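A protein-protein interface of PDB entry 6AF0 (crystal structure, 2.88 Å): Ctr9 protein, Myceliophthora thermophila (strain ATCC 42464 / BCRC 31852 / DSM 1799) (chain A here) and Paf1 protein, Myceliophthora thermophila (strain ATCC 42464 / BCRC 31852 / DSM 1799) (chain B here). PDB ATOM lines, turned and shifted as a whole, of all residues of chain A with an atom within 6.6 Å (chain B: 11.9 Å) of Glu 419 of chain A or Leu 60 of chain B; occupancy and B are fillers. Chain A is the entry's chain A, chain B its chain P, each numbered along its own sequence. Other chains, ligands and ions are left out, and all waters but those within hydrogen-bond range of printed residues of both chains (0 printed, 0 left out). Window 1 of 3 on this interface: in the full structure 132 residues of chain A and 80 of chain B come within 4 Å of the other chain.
Of the printed residues of chain B, Tyr 351 of chain A touches Ala 61 (3.4 Å).
Of chain B, only Leu 60 and Gln 64 come within 4 Å of Pro 386 of chain A.
Phe 389 of chain A touches one residue of chain B.
No residue of chain B comes within 4 Å of Asn 417 of chain A.
No residue of chain B comes within 4 Å of Tyr 418 of chain A.
Leu 423 of chain A touches one residue of chain B.
Of the printed residues of chain A, Tyr 51 of chain B touches Ile 422.
Of the printed residues of chain A, Ala 57 of chain B touches Phe 389 (3.6 Å).
The nearest residue of chain A that does not touch Leu 60 of chain B is Asn 417 of chain A (4.2 Å).
The nearest printed residue of chain B that does not touch Tyr 384 of chain A is Pro 65 of chain B (5.5 Å).
Ala 61 of chain B touches Tyr 351 of chain A (CB to OH, 3.4 Å).
Tyr 384 of chain A touches Ala 61 of chain B (OH to O, 3.96 Å).
Tyr 384 of chain A touches Gln 64 of chain B (OH to CB, 3.8 Å).
Leu 385 of chain A touches Leu 60 of chain B.
Pro 386 of chain A touches Leu 60 of chain B (CG to CD1, 3.7 Å).
Pro 386 of chain A touches Gln 64 of chain B (CG to CG, 3.5 Å).
Ala 57 of chain B touches Phe 389 of chain A.
Leu 60 of chain B touches Glu 419 of chain A.
Ile 422 of chain A touches Tyr 51 of chain B.
Leu 46 of chain B touches Leu 423 of chain A (CD1 to CD1, 3.6 Å).
OD1 of Asn 417 of chain A lies close to OE1 of Glu 419 of chain A (2.9 Å).
Of the 19 printed residues of chain B, 6 touch a printed residue of chain A.
Hydrophobic or aromatic side chains of chain B within 4 Å of the printed part of chain A: Leu 46, Tyr 51, Ala 57, Leu 60 and Ala 61.
Along chain B the printed residues that touch a printed residue of chain A span positions 46 to 64.
Of the 17 printed residues of chain A, 8 touch a printed residue of chain B.
Printed residues of chain A that touch a printed residue of chain B: Tyr 351, Tyr 384, Leu 385, Pro 386, Phe 389, Glu 419, Ile 422 and Leu 423.
Hydrophobic or aromatic side chains of chain A within 4 Å of the printed part of chain B: Tyr 351, Tyr 384, Leu 385, Pro 386, Phe 389, Ile 422 and Leu 423.
Among the printed residues, no Asp or Glu carboxylate lies within 4 Å of a Lys or Arg side-chain nitrogen of the other chain.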
ATOM      1  N   TYR A 351     -15.799   3.297  -6.254  1.00  0.00           N
ATOM      2  CA  TYR A 351     -17.144   3.766  -6.505  1.00  0.00           C
ATOM      3  C   TYR A 351     -18.170   2.755  -5.997  1.00  0.00           C
ATOM      4  O   TYR A 351     -19.123   3.130  -5.357  1.00  0.00           O
ATOM      5  CB  TYR A 351     -17.354   4.051  -7.979  1.00  0.00           C
ATOM      6  CG  TYR A 351     -18.740   4.540  -8.250  1.00  0.00           C
ATOM      7  CD1 TYR A 351     -19.145   5.795  -7.817  1.00  0.00           C
ATOM      8  CD2 TYR A 351     -19.669   3.747  -8.915  1.00  0.00           C
ATOM      9  CE1 TYR A 351     -20.431   6.256  -8.059  1.00  0.00           C
ATOM     10  CE2 TYR A 351     -20.949   4.211  -9.177  1.00  0.00           C
ATOM     11  CZ  TYR A 351     -21.323   5.466  -8.733  1.00  0.00           C
ATOM     12  OH  TYR A 351     -22.577   5.959  -8.938  1.00  0.00           O
ATOM     13  N   TYR A 384     -14.154  10.625 -12.150  1.00  0.00           N
ATOM     14  CA  TYR A 384     -15.343   9.818 -12.371  1.00  0.00           C
ATOM     15  C   TYR A 384     -16.570  10.629 -11.976  1.00  0.00           C
ATOM     16  O   TYR A 384     -16.818  10.867 -10.779  1.00  0.00           O
ATOM     17  CB  TYR A 384     -15.265   8.510 -11.571  1.00  0.00           C
ATOM     18  CG  TYR A 384     -16.169   7.413 -12.093  1.00  0.00           C
ATOM     19  CD1 TYR A 384     -16.077   6.957 -13.400  1.00  0.00           C
ATOM     20  CD2 TYR A 384     -17.118   6.832 -11.273  1.00  0.00           C
ATOM     21  CE1 TYR A 384     -16.928   5.969 -13.876  1.00  0.00           C
ATOM     22  CE2 TYR A 384     -17.956   5.840 -11.727  1.00  0.00           C
ATOM     23  CZ  TYR A 384     -17.864   5.411 -13.025  1.00  0.00           C
ATOM     24  OH  TYR A 384     -18.737   4.422 -13.410  1.00  0.00           O
ATOM     25  N   LEU A 385     -17.340  11.023 -12.988  1.00  0.00           N
ATOM     26  CA  LEU A 385     -18.547  11.819 -12.788  1.00  0.00           C
ATOM     27  C   LEU A 385     -19.539  11.271 -11.730  1.00  0.00           C
ATOM     28  O   LEU A 385     -20.025  12.008 -10.881  1.00  0.00           O
ATOM     29  CB  LEU A 385     -19.227  12.034 -14.127  1.00  0.00           C
ATOM     30  CG  LEU A 385     -20.257  13.157 -14.143  1.00  0.00           C
ATOM     31  CD1 LEU A 385     -20.303  13.844 -15.501  1.00  0.00           C
ATOM     32  CD2 LEU A 385     -21.630  12.619 -13.782  1.00  0.00           C
ATOM     33  N   PRO A 386     -19.835   9.984 -11.771  1.00  0.00           N
ATOM     34  CA  PRO A 386     -20.696   9.482 -10.707  1.00  0.00           C
ATOM     35  C   PRO A 386     -20.103   9.602  -9.298  1.00  0.00           C
ATOM     36  O   PRO A 386     -20.857   9.690  -8.308  1.00  0.00           O
ATOM     37  CB  PRO A 386     -20.894   7.996 -11.085  1.00  0.00           C
ATOM     38  CG  PRO A 386     -20.660   7.951 -12.553  1.00  0.00           C
ATOM     39  CD  PRO A 386     -19.615   8.987 -12.833  1.00  0.00           C
ATOM     40  N   ALA A 387     -18.780   9.558  -9.199  1.00  0.00           N
ATOM     41  CA  ALA A 387     -18.123   9.585  -7.885  1.00  0.00           C
ATOM     42  C   ALA A 387     -18.238  10.982  -7.281  1.00  0.00           C
ATOM     43  O   ALA A 387     -18.476  11.162  -6.071  1.00  0.00           O
ATOM     44  CB  ALA A 387     -16.662   9.189  -8.013  1.00  0.00           C
ATOM     45  N   PHE A 389     -20.557  13.071  -8.053  1.00  0.00           N
ATOM     46  CA  PHE A 389     -21.934  13.266  -7.701  1.00  0.00           C
ATOM     47  C   PHE A 389     -22.192  12.647  -6.338  1.00  0.00           C
ATOM     48  O   PHE A 389     -22.821  13.265  -5.496  1.00  0.00           O
ATOM     49  CB  PHE A 389     -22.838  12.688  -8.784  1.00  0.00           C
ATOM     50  CG  PHE A 389     -24.313  12.853  -8.515  1.00  0.00           C
ATOM     51  CD1 PHE A 389     -25.058  11.817  -7.970  1.00  0.00           C
ATOM     52  CD2 PHE A 389     -24.951  14.036  -8.820  1.00  0.00           C
ATOM     53  CE1 PHE A 389     -26.408  11.964  -7.742  1.00  0.00           C
ATOM     54  CE2 PHE A 389     -26.305  14.194  -8.579  1.00  0.00           C
ATOM     55  CZ  PHE A 389     -27.033  13.156  -8.041  1.00  0.00           C
ATOM     56  N   LEU A 408     -21.139  20.705  -7.359  1.00  0.00           N
ATOM     57  CA  LEU A 408     -22.196  20.701  -8.369  1.00  0.00           C
ATOM     58  C   LEU A 408     -21.895  21.763  -9.412  1.00  0.00           C
ATOM     59  O   LEU A 408     -21.942  21.505 -10.608  1.00  0.00           O
ATOM     60  CB  LEU A 408     -23.558  20.941  -7.722  1.00  0.00           C
ATOM     61  CG  LEU A 408     -24.031  19.836  -6.765  1.00  0.00           C
ATOM     62  CD1 LEU A 408     -24.998  20.364  -5.711  1.00  0.00           C
ATOM     63  CD2 LEU A 408     -24.664  18.688  -7.530  1.00  0.00           C
ATOM     64  N   MET A 411     -19.056  20.692 -11.544  1.00  0.00           N
ATOM     65  CA  MET A 411     -19.581  19.708 -12.508  1.00  0.00           C
ATOM     66  C   MET A 411     -20.345  20.283 -13.692  1.00  0.00           C
ATOM     67  O   MET A 411     -20.144  19.867 -14.830  1.00  0.00           O
ATOM     68  CB  MET A 411     -20.570  18.789 -11.815  1.00  0.00           C
ATOM     69  CG  MET A 411     -20.001  17.524 -11.241  1.00  0.00           C
ATOM     70  SD  MET A 411     -21.414  16.464 -10.966  1.00  0.00           S
ATOM     71  CE  MET A 411     -21.034  15.899  -9.332  1.00  0.00           C
ATOM     72  N   LYS A 416     -23.100  19.898 -18.874  1.00  0.00           N
ATOM     73  CA  LYS A 416     -24.463  20.145 -18.402  1.00  0.00           C
ATOM     74  C   LYS A 416     -25.138  18.879 -17.907  1.00  0.00           C
ATOM     75  O   LYS A 416     -26.216  18.493 -18.371  1.00  0.00           O
ATOM     76  CB  LYS A 416     -25.300  20.885 -19.460  1.00  0.00           C
ATOM     77  CG  LYS A 416     -25.096  22.405 -19.467  1.00  0.00           C
ATOM     78  CD  LYS A 416     -24.685  22.977 -18.097  1.00  0.00           C
ATOM     79  CE  LYS A 416     -24.782  24.495 -17.998  1.00  0.00           C
ATOM     80  NZ  LYS A 416     -26.158  25.024 -18.242  1.00  0.00           N
ATOM     81  N   ASN A 417     -24.509  18.258 -16.916  1.00  0.00           N
ATOM     82  CA  ASN A 417     -25.031  17.028 -16.367  1.00  0.00           C
ATOM     83  C   ASN A 417     -26.409  17.210 -15.752  1.00  0.00           C
ATOM     84  O   ASN A 417     -26.598  18.036 -14.868  1.00  0.00           O
ATOM     85  CB  ASN A 417     -24.116  16.470 -15.300  1.00  0.00           C
ATOM     86  CG  ASN A 417     -24.710  15.253 -14.628  1.00  0.00           C
ATOM     87  OD1 ASN A 417     -25.667  14.665 -15.131  1.00  0.00           O
ATOM     88  ND2 ASN A 417     -24.161  14.876 -13.488  1.00  0.00           N
ATOM     89  N   TYR A 418     -27.353  16.393 -16.194  1.00  0.00           N
ATOM     90  CA  TYR A 418     -28.723  16.454 -15.701  1.00  0.00           C
ATOM     91  C   TYR A 418     -28.797  16.347 -14.170  1.00  0.00           C
ATOM     92  O   TYR A 418     -29.371  17.198 -13.512  1.00  0.00           O
ATOM     93  CB  TYR A 418     -29.556  15.354 -16.378  1.00  0.00           C
ATOM     94  CG  TYR A 418     -30.932  15.166 -15.817  1.00  0.00           C
ATOM     95  CD1 TYR A 418     -31.135  14.407 -14.665  1.00  0.00           C
ATOM     96  CD2 TYR A 418     -32.038  15.735 -16.437  1.00  0.00           C
ATOM     97  CE1 TYR A 418     -32.400  14.225 -14.144  1.00  0.00           C
ATOM     98  CE2 TYR A 418     -33.315  15.559 -15.922  1.00  0.00           C
ATOM     99  CZ  TYR A 418     -33.483  14.806 -14.776  1.00  0.00           C
ATOM    100  OH  TYR A 418     -34.737  14.623 -14.254  1.00  0.00           O
ATOM    101  N   GLU A 419     -28.204  15.310 -13.613  1.00  0.00           N
ATOM    102  CA  GLU A 419     -28.312  15.033 -12.175  1.00  0.00           C
ATOM    103  C   GLU A 419     -27.734  16.135 -11.285  1.00  0.00           C
ATOM    104  O   GLU A 419     -28.239  16.397 -10.195  1.00  0.00           O
ATOM    105  CB  GLU A 419     -27.618  13.713 -11.832  1.00  0.00           C
ATOM    106  CG  GLU A 419     -28.412  12.448 -12.171  1.00  0.00           C
ATOM    107  CD  GLU A 419     -28.283  11.957 -13.625  1.00  0.00           C
ATOM    108  OE1 GLU A 419     -27.514  12.525 -14.433  1.00  0.00           O
ATOM    109  OE2 GLU A 419     -28.970  10.969 -13.975  1.00  0.00           O
ATOM    110  N   ALA A 420     -26.645  16.748 -11.737  1.00  0.00           N
ATOM    111  CA  ALA A 420     -26.084  17.912 -11.053  1.00  0.00           C
ATOM    112  C   ALA A 420     -27.114  19.053 -11.112  1.00  0.00           C
ATOM    113  O   ALA A 420     -27.582  19.530 -10.073  1.00  0.00           O
ATOM    114  CB  ALA A 420     -24.753  18.322 -11.680  1.00  0.00           C
ATOM    115  N   MET A 421     -27.505  19.420 -12.335  1.00  0.00           N
ATOM    116  CA  MET A 421     -28.455  20.503 -12.571  1.00  0.00           C
ATOM    117  C   MET A 421     -29.701  20.432 -11.684  1.00  0.00           C
ATOM    118  O   MET A 421     -30.109  21.420 -11.094  1.00  0.00           O
ATOM    119  CB  MET A 421     -28.871  20.531 -14.048  1.00  0.00           C
ATOM    120  CG  MET A 421     -27.774  20.986 -14.996  1.00  0.00           C
ATOM    121  SD  MET A 421     -28.404  21.832 -16.453  1.00  0.00           S
ATOM    122  CE  MET A 421     -29.521  20.610 -17.130  1.00  0.00           C
ATOM    123  N   ILE A 422     -30.315  19.268 -11.599  1.00  0.00           N
ATOM    124  CA  ILE A 422     -31.543  19.131 -10.819  1.00  0.00           C
ATOM    125  C   ILE A 422     -31.268  19.263  -9.332  1.00  0.00           C
ATOM    126  O   ILE A 422     -32.096  19.762  -8.595  1.00  0.00           O
ATOM    127  CB  ILE A 422     -32.292  17.798 -11.087  1.00  0.00           C
ATOM    128  CG1 ILE A 422     -33.590  17.745 -10.278  1.00  0.00           C
ATOM    129  CG2 ILE A 422     -31.448  16.582 -10.724  1.00  0.00           C
ATOM    130  CD1 ILE A 422     -34.536  16.638 -10.691  1.00  0.00           C
ATOM    131  N   LEU A 423     -30.115  18.799  -8.882  1.00  0.00           N
ATOM    132  CA  LEU A 423     -29.815  18.838  -7.450  1.00  0.00           C
ATOM    133  C   LEU A 423     -29.425  20.235  -7.022  1.00  0.00           C
ATOM    134  O   LEU A 423     -29.851  20.730  -5.974  1.00  0.00           O
ATOM    135  CB  LEU A 423     -28.674  17.889  -7.098  1.00  0.00           C
ATOM    136  CG  LEU A 423     -28.355  17.843  -5.605  1.00  0.00           C
ATOM    137  CD1 LEU A 423     -29.609  17.594  -4.783  1.00  0.00           C
ATOM    138  CD2 LEU A 423     -27.313  16.769  -5.309  1.00  0.00           C
ATOM    139  N   LEU A 424     -28.588  20.863  -7.836  1.00  0.00           N
ATOM    140  CA  LEU A 424     -28.150  22.199  -7.544  1.00  0.00           C
ATOM    141  C   LEU A 424     -29.367  23.128  -7.519  1.00  0.00           C
ATOM    142  O   LEU A 424     -29.631  23.766  -6.505  1.00  0.00           O
ATOM    143  CB  LEU A 424     -27.074  22.641  -8.540  1.00  0.00           C
ATOM    144  CG  LEU A 424     -26.371  23.976  -8.243  1.00  0.00           C
ATOM    145  CD1 LEU A 424     -25.722  24.021  -6.856  1.00  0.00           C
ATOM    146  CD2 LEU A 424     -25.343  24.244  -9.335  1.00  0.00           C
ATOM    147  N   LEU B  46     -34.850  18.047  -0.094  1.00  0.00           N
ATOM    148  CA  LEU B  46     -33.574  17.348  -0.111  1.00  0.00           C
ATOM    149  C   LEU B  46     -33.488  16.504   1.158  1.00  0.00           C
ATOM    150  O   LEU B  46     -32.933  15.396   1.125  1.00  0.00           O
ATOM    151  CB  LEU B  46     -32.391  18.324  -0.212  1.00  0.00           C
ATOM    152  CG  LEU B  46     -32.173  19.132  -1.513  1.00  0.00           C
ATOM    153  CD1 LEU B  46     -32.483  18.334  -2.769  1.00  0.00           C
ATOM    154  CD2 LEU B  46     -32.987  20.409  -1.528  1.00  0.00           C
ATOM    155  N   GLY B  49     -35.044  11.917   1.574  1.00  0.00           N
ATOM    156  CA  GLY B  49     -33.847  11.329   0.956  1.00  0.00           C
ATOM    157  C   GLY B  49     -33.775  11.086  -0.548  1.00  0.00           C
ATOM    158  O   GLY B  49     -32.695  10.792  -1.043  1.00  0.00           O
ATOM    159  N   GLN B  50     -34.881  11.227  -1.285  1.00  0.00           N
ATOM    160  CA  GLN B  50     -34.951  10.744  -2.690  1.00  0.00           C
ATOM    161  C   GLN B  50     -33.810  11.266  -3.609  1.00  0.00           C
ATOM    162  O   GLN B  50     -33.232  10.512  -4.409  1.00  0.00           O
ATOM    163  CB  GLN B  50     -36.352  10.996  -3.315  1.00  0.00           C
ATOM    164  CG  GLN B  50     -36.486  12.255  -4.178  1.00  0.00           C
ATOM    165  CD  GLN B  50     -37.660  12.219  -5.153  1.00  0.00           C
ATOM    166  OE1 GLN B  50     -38.077  11.151  -5.605  1.00  0.00           O
ATOM    167  NE2 GLN B  50     -38.184  13.399  -5.501  1.00  0.00           N
ATOM    168  N   TYR B  51     -33.470  12.539  -3.475  1.00  0.00           N
ATOM    169  CA  TYR B  51     -32.474  13.150  -4.349  1.00  0.00           C
ATOM    170  C   TYR B  51     -31.039  12.859  -3.903  1.00  0.00           C
ATOM    171  O   TYR B  51     -30.096  13.063  -4.662  1.00  0.00           O
ATOM    172  CB  TYR B  51     -32.677  14.658  -4.385  1.00  0.00           C
ATOM    173  CG  TYR B  51     -33.816  15.112  -5.249  1.00  0.00           C
ATOM    174  CD1 TYR B  51     -33.733  15.014  -6.619  1.00  0.00           C
ATOM    175  CD2 TYR B  51     -34.975  15.660  -4.691  1.00  0.00           C
ATOM    176  CE1 TYR B  51     -34.768  15.438  -7.428  1.00  0.00           C
ATOM    177  CE2 TYR B  51     -36.022  16.084  -5.489  1.00  0.00           C
ATOM    178  CZ  TYR B  51     -35.913  15.972  -6.861  1.00  0.00           C
ATOM    179  OH  TYR B  51     -36.946  16.398  -7.663  1.00  0.00           O
ATOM    180  N   THR B  52     -30.885  12.442  -2.649  1.00  0.00           N
ATOM    181  CA  THR B  52     -29.576  12.133  -2.051  1.00  0.00           C
ATOM    182  C   THR B  52     -29.307  10.629  -1.964  1.00  0.00           C
ATOM    183  O   THR B  52     -28.231  10.213  -1.550  1.00  0.00           O
ATOM    184  CB  THR B  52     -29.454  12.733  -0.622  1.00  0.00           C
ATOM    185  OG1 THR B  52     -30.507  12.244   0.230  1.00  0.00           O
ATOM    186  CG2 THR B  52     -29.513  14.246  -0.673  1.00  0.00           C
ATOM    187  N   ALA B  53     -30.294   9.815  -2.335  1.00  0.00           N
ATOM    188  CA  ALA B  53     -30.157   8.355  -2.312  1.00  0.00           C
ATOM    189  C   ALA B  53     -29.296   7.926  -3.475  1.00  0.00           C
ATOM    190  O   ALA B  53     -29.419   8.495  -4.566  1.00  0.00           O
ATOM    191  CB  ALA B  53     -31.517   7.682  -2.426  1.00  0.00           C
ATOM    192  N   PRO B  54     -28.447   6.905  -3.267  1.00  0.00           N
ATOM    193  CA  PRO B  54     -27.651   6.333  -4.357  1.00  0.00           C
ATOM    194  C   PRO B  54     -28.503   6.065  -5.581  1.00  0.00           C
ATOM    195  O   PRO B  54     -28.146   6.482  -6.691  1.00  0.00           O
ATOM    196  CB  PRO B  54     -27.137   5.020  -3.770  1.00  0.00           C
ATOM    197  CG  PRO B  54     -27.090   5.259  -2.308  1.00  0.00           C
ATOM    198  CD  PRO B  54     -28.246   6.173  -2.006  1.00  0.00           C
ATOM    199  N   GLY B  55     -29.650   5.427  -5.356  1.00  0.00           N
ATOM    200  CA  GLY B  55     -30.570   5.054  -6.427  1.00  0.00           C
ATOM    201  C   GLY B  55     -30.695   6.087  -7.521  1.00  0.00           C
ATOM    202  O   GLY B  55     -30.703   5.754  -8.696  1.00  0.00           O
ATOM    203  N   PHE B  56     -30.758   7.352  -7.140  1.00  0.00           N
ATOM    204  CA  PHE B  56     -31.048   8.406  -8.096  1.00  0.00           C
ATOM    205  C   PHE B  56     -29.912   8.548  -9.097  1.00  0.00           C
ATOM    206  O   PHE B  56     -30.093   9.053 -10.201  1.00  0.00           O
ATOM    207  CB  PHE B  56     -31.287   9.707  -7.356  1.00  0.00           C
ATOM    208  CG  PHE B  56     -31.841  10.776  -8.224  1.00  0.00           C
ATOM    209  CD1 PHE B  56     -33.187  10.784  -8.542  1.00  0.00           C
ATOM    210  CD2 PHE B  56     -31.020  11.761  -8.740  1.00  0.00           C
ATOM    211  CE1 PHE B  56     -33.714  11.758  -9.357  1.00  0.00           C
ATOM    212  CE2 PHE B  56     -31.529  12.738  -9.559  1.00  0.00           C
ATOM    213  CZ  PHE B  56     -32.882  12.736  -9.869  1.00  0.00           C
ATOM    214  N   ALA B  57     -28.737   8.079  -8.683  1.00  0.00           N
ATOM    215  CA  ALA B  57     -27.511   8.131  -9.478  1.00  0.00           C
ATOM    216  C   ALA B  57     -27.230   6.833 -10.226  1.00  0.00           C
ATOM    217  O   ALA B  57     -26.286   6.786 -11.010  1.00  0.00           O
ATOM    218  CB  ALA B  57     -26.329   8.446  -8.568  1.00  0.00           C
ATOM    219  N   SER B  58     -28.023   5.787  -9.973  1.00  0.00           N
ATOM    220  CA  SER B  58     -27.754   4.477 -10.566  1.00  0.00           C
ATOM    221  C   SER B  58     -27.886   4.499 -12.107  1.00  0.00           C
ATOM    222  O   SER B  58     -27.059   3.935 -12.827  1.00  0.00           O
ATOM    223  CB  SER B  58     -28.558   3.345  -9.898  1.00  0.00           C
ATOM    224  OG  SER B  58     -29.926   3.611  -9.868  1.00  0.00           O
ATOM    225  N   ARG B  59     -28.877   5.196 -12.627  1.00  0.00           N
ATOM    226  CA  ARG B  59     -28.944   5.362 -14.071  1.00  0.00           C
ATOM    227  C   ARG B  59     -27.676   6.045 -14.582  1.00  0.00           C
ATOM    228  O   ARG B  59     -27.028   5.569 -15.499  1.00  0.00           O
ATOM    229  CB  ARG B  59     -30.189   6.169 -14.450  1.00  0.00           C
ATOM    230  CG  ARG B  59     -30.324   6.485 -15.932  1.00  0.00           C
ATOM    231  CD  ARG B  59     -31.788   6.592 -16.313  1.00  0.00           C
ATOM    232  NE  ARG B  59     -32.454   5.278 -16.391  1.00  0.00           N
ATOM    233  CZ  ARG B  59     -33.775   5.085 -16.518  1.00  0.00           C
ATOM    234  NH1 ARG B  59     -34.613   6.121 -16.567  1.00  0.00           N
ATOM    235  NH2 ARG B  59     -34.273   3.849 -16.588  1.00  0.00           N
ATOM    236  N   LEU B  60     -27.321   7.157 -13.959  1.00  0.00           N
ATOM    237  CA  LEU B  60     -26.152   7.954 -14.349  1.00  0.00           C
ATOM    238  C   LEU B  60     -24.873   7.129 -14.278  1.00  0.00           C
ATOM    239  O   LEU B  60     -23.935   7.337 -15.056  1.00  0.00           O
ATOM    240  CB  LEU B  60     -26.046   9.178 -13.427  1.00  0.00           C
ATOM    241  CG  LEU B  60     -25.011  10.310 -13.605  1.00  0.00           C
ATOM    242  CD1 LEU B  60     -23.743  10.044 -12.810  1.00  0.00           C
ATOM    243  CD2 LEU B  60     -24.702  10.578 -15.073  1.00  0.00           C
ATOM    244  N   ALA B  61     -24.843   6.190 -13.341  1.00  0.00           N
ATOM    245  CA  ALA B  61     -23.696   5.315 -13.167  1.00  0.00           C
ATOM    246  C   ALA B  61     -23.589   4.263 -14.247  1.00  0.00           C
ATOM    247  O   ALA B  61     -22.485   3.840 -14.556  1.00  0.00           O
ATOM    248  CB  ALA B  61     -23.754   4.637 -11.818  1.00  0.00           C
ATOM    249  N   ARG B  62     -24.733   3.833 -14.793  1.00  0.00           N
ATOM    250  CA  ARG B  62     -24.796   2.730 -15.772  1.00  0.00           C
ATOM    251  C   ARG B  62     -24.500   3.215 -17.165  1.00  0.00           C
ATOM    252  O   ARG B  62     -23.904   2.474 -17.949  1.00  0.00           O
ATOM    253  CB  ARG B  62     -26.164   2.048 -15.773  1.00  0.00           C
ATOM    254  CG  ARG B  62     -26.480   1.263 -14.491  1.00  0.00           C
ATOM    255  CD  ARG B  62     -27.945   0.826 -14.399  1.00  0.00           C
ATOM    256  NE  ARG B  62     -28.593   0.994 -15.701  1.00  0.00           N
ATOM    257  CZ  ARG B  62     -29.654   1.757 -15.952  1.00  0.00           C
ATOM    258  NH1 ARG B  62     -30.288   2.406 -14.972  1.00  0.00           N
ATOM    259  NH2 ARG B  62     -30.108   1.838 -17.207  1.00  0.00           N
ATOM    260  N   GLU B  63     -24.902   4.450 -17.477  1.00  0.00           N
ATOM    261  CA  GLU B  63     -24.681   4.995 -18.815  1.00  0.00           C
ATOM    262  C   GLU B  63     -23.245   5.491 -18.954  1.00  0.00           C
ATOM    263  O   GLU B  63     -22.850   6.059 -19.965  1.00  0.00           O
ATOM    264  CB  GLU B  63     -25.726   6.060 -19.175  1.00  0.00           C
ATOM    265  CG  GLU B  63     -25.434   7.485 -18.735  1.00  0.00           C
ATOM    266  CD  GLU B  63     -26.460   8.479 -19.278  1.00  0.00           C
ATOM    267  OE1 GLU B  63     -27.452   8.036 -19.937  1.00  0.00           O
ATOM    268  OE2 GLU B  63     -26.265   9.703 -19.042  1.00  0.00           O
ATOM    269  N   GLN B  64     -22.447   5.261 -17.928  1.00  0.00           N
ATOM    270  CA  GLN B  64     -21.030   5.526 -18.024  1.00  0.00           C
ATOM    271  C   GLN B  64     -20.379   4.404 -18.811  1.00  0.00           C
ATOM    272  O   GLN B  64     -20.624   3.219 -18.540  1.00  0.00           O
ATOM    273  CB  GLN B  64     -20.410   5.635 -16.627  1.00  0.00           C
ATOM    274  CG  GLN B  64     -20.724   6.932 -15.907  1.00  0.00           C
ATOM    275  CD  GLN B  64     -20.121   8.125 -16.597  1.00  0.00           C
ATOM    276  OE1 GLN B  64     -18.921   8.138 -16.888  1.00  0.00           O
ATOM    277  NE2 GLN B  64     -20.945   9.128 -16.890  1.00  0.00           N
ATOM    278  N   PRO B  65     -19.521   4.767 -19.768  1.00  0.00           N
ATOM    279  CA  PRO B  65     -18.773   3.786 -20.563  1.00  0.00           C
ATOM    280  C   PRO B  65     -18.093   2.748 -19.698  1.00  0.00           C
ATOM    281  O   PRO B  65     -17.575   3.079 -18.628  1.00  0.00           O
ATOM    282  CB  PRO B  65     -17.729   4.632 -21.286  1.00  0.00           C
ATOM    283  CG  PRO B  65     -18.381   5.961 -21.410  1.00  0.00           C
ATOM    284  CD  PRO B  65     -19.148   6.140 -20.120  1.00  0.00           C
ATOM    285  N   LEU B  66     -18.139   1.497 -20.146  1.00  0.00           N
ATOM    286  CA  LEU B  66     -17.426   0.426 -19.467  1.00  0.00           C
ATOM    287  C   LEU B  66     -15.983   0.464 -19.864  1.00  0.00           C
ATOM    288  O   LEU B  66     -15.648   0.702 -21.037  1.00  0.00           O
ATOM    289  CB  LEU B  66     -17.966  -0.940 -19.841  1.00  0.00           C
ATOM    290  CG  LEU B  66     -19.333  -1.319 -19.315  1.00  0.00           C
ATOM    291  CD1 LEU B  66     -19.628  -2.720 -19.808  1.00  0.00           C
ATOM    292  CD2 LEU B  66     -19.363  -1.301 -17.812  1.00  0.00           C
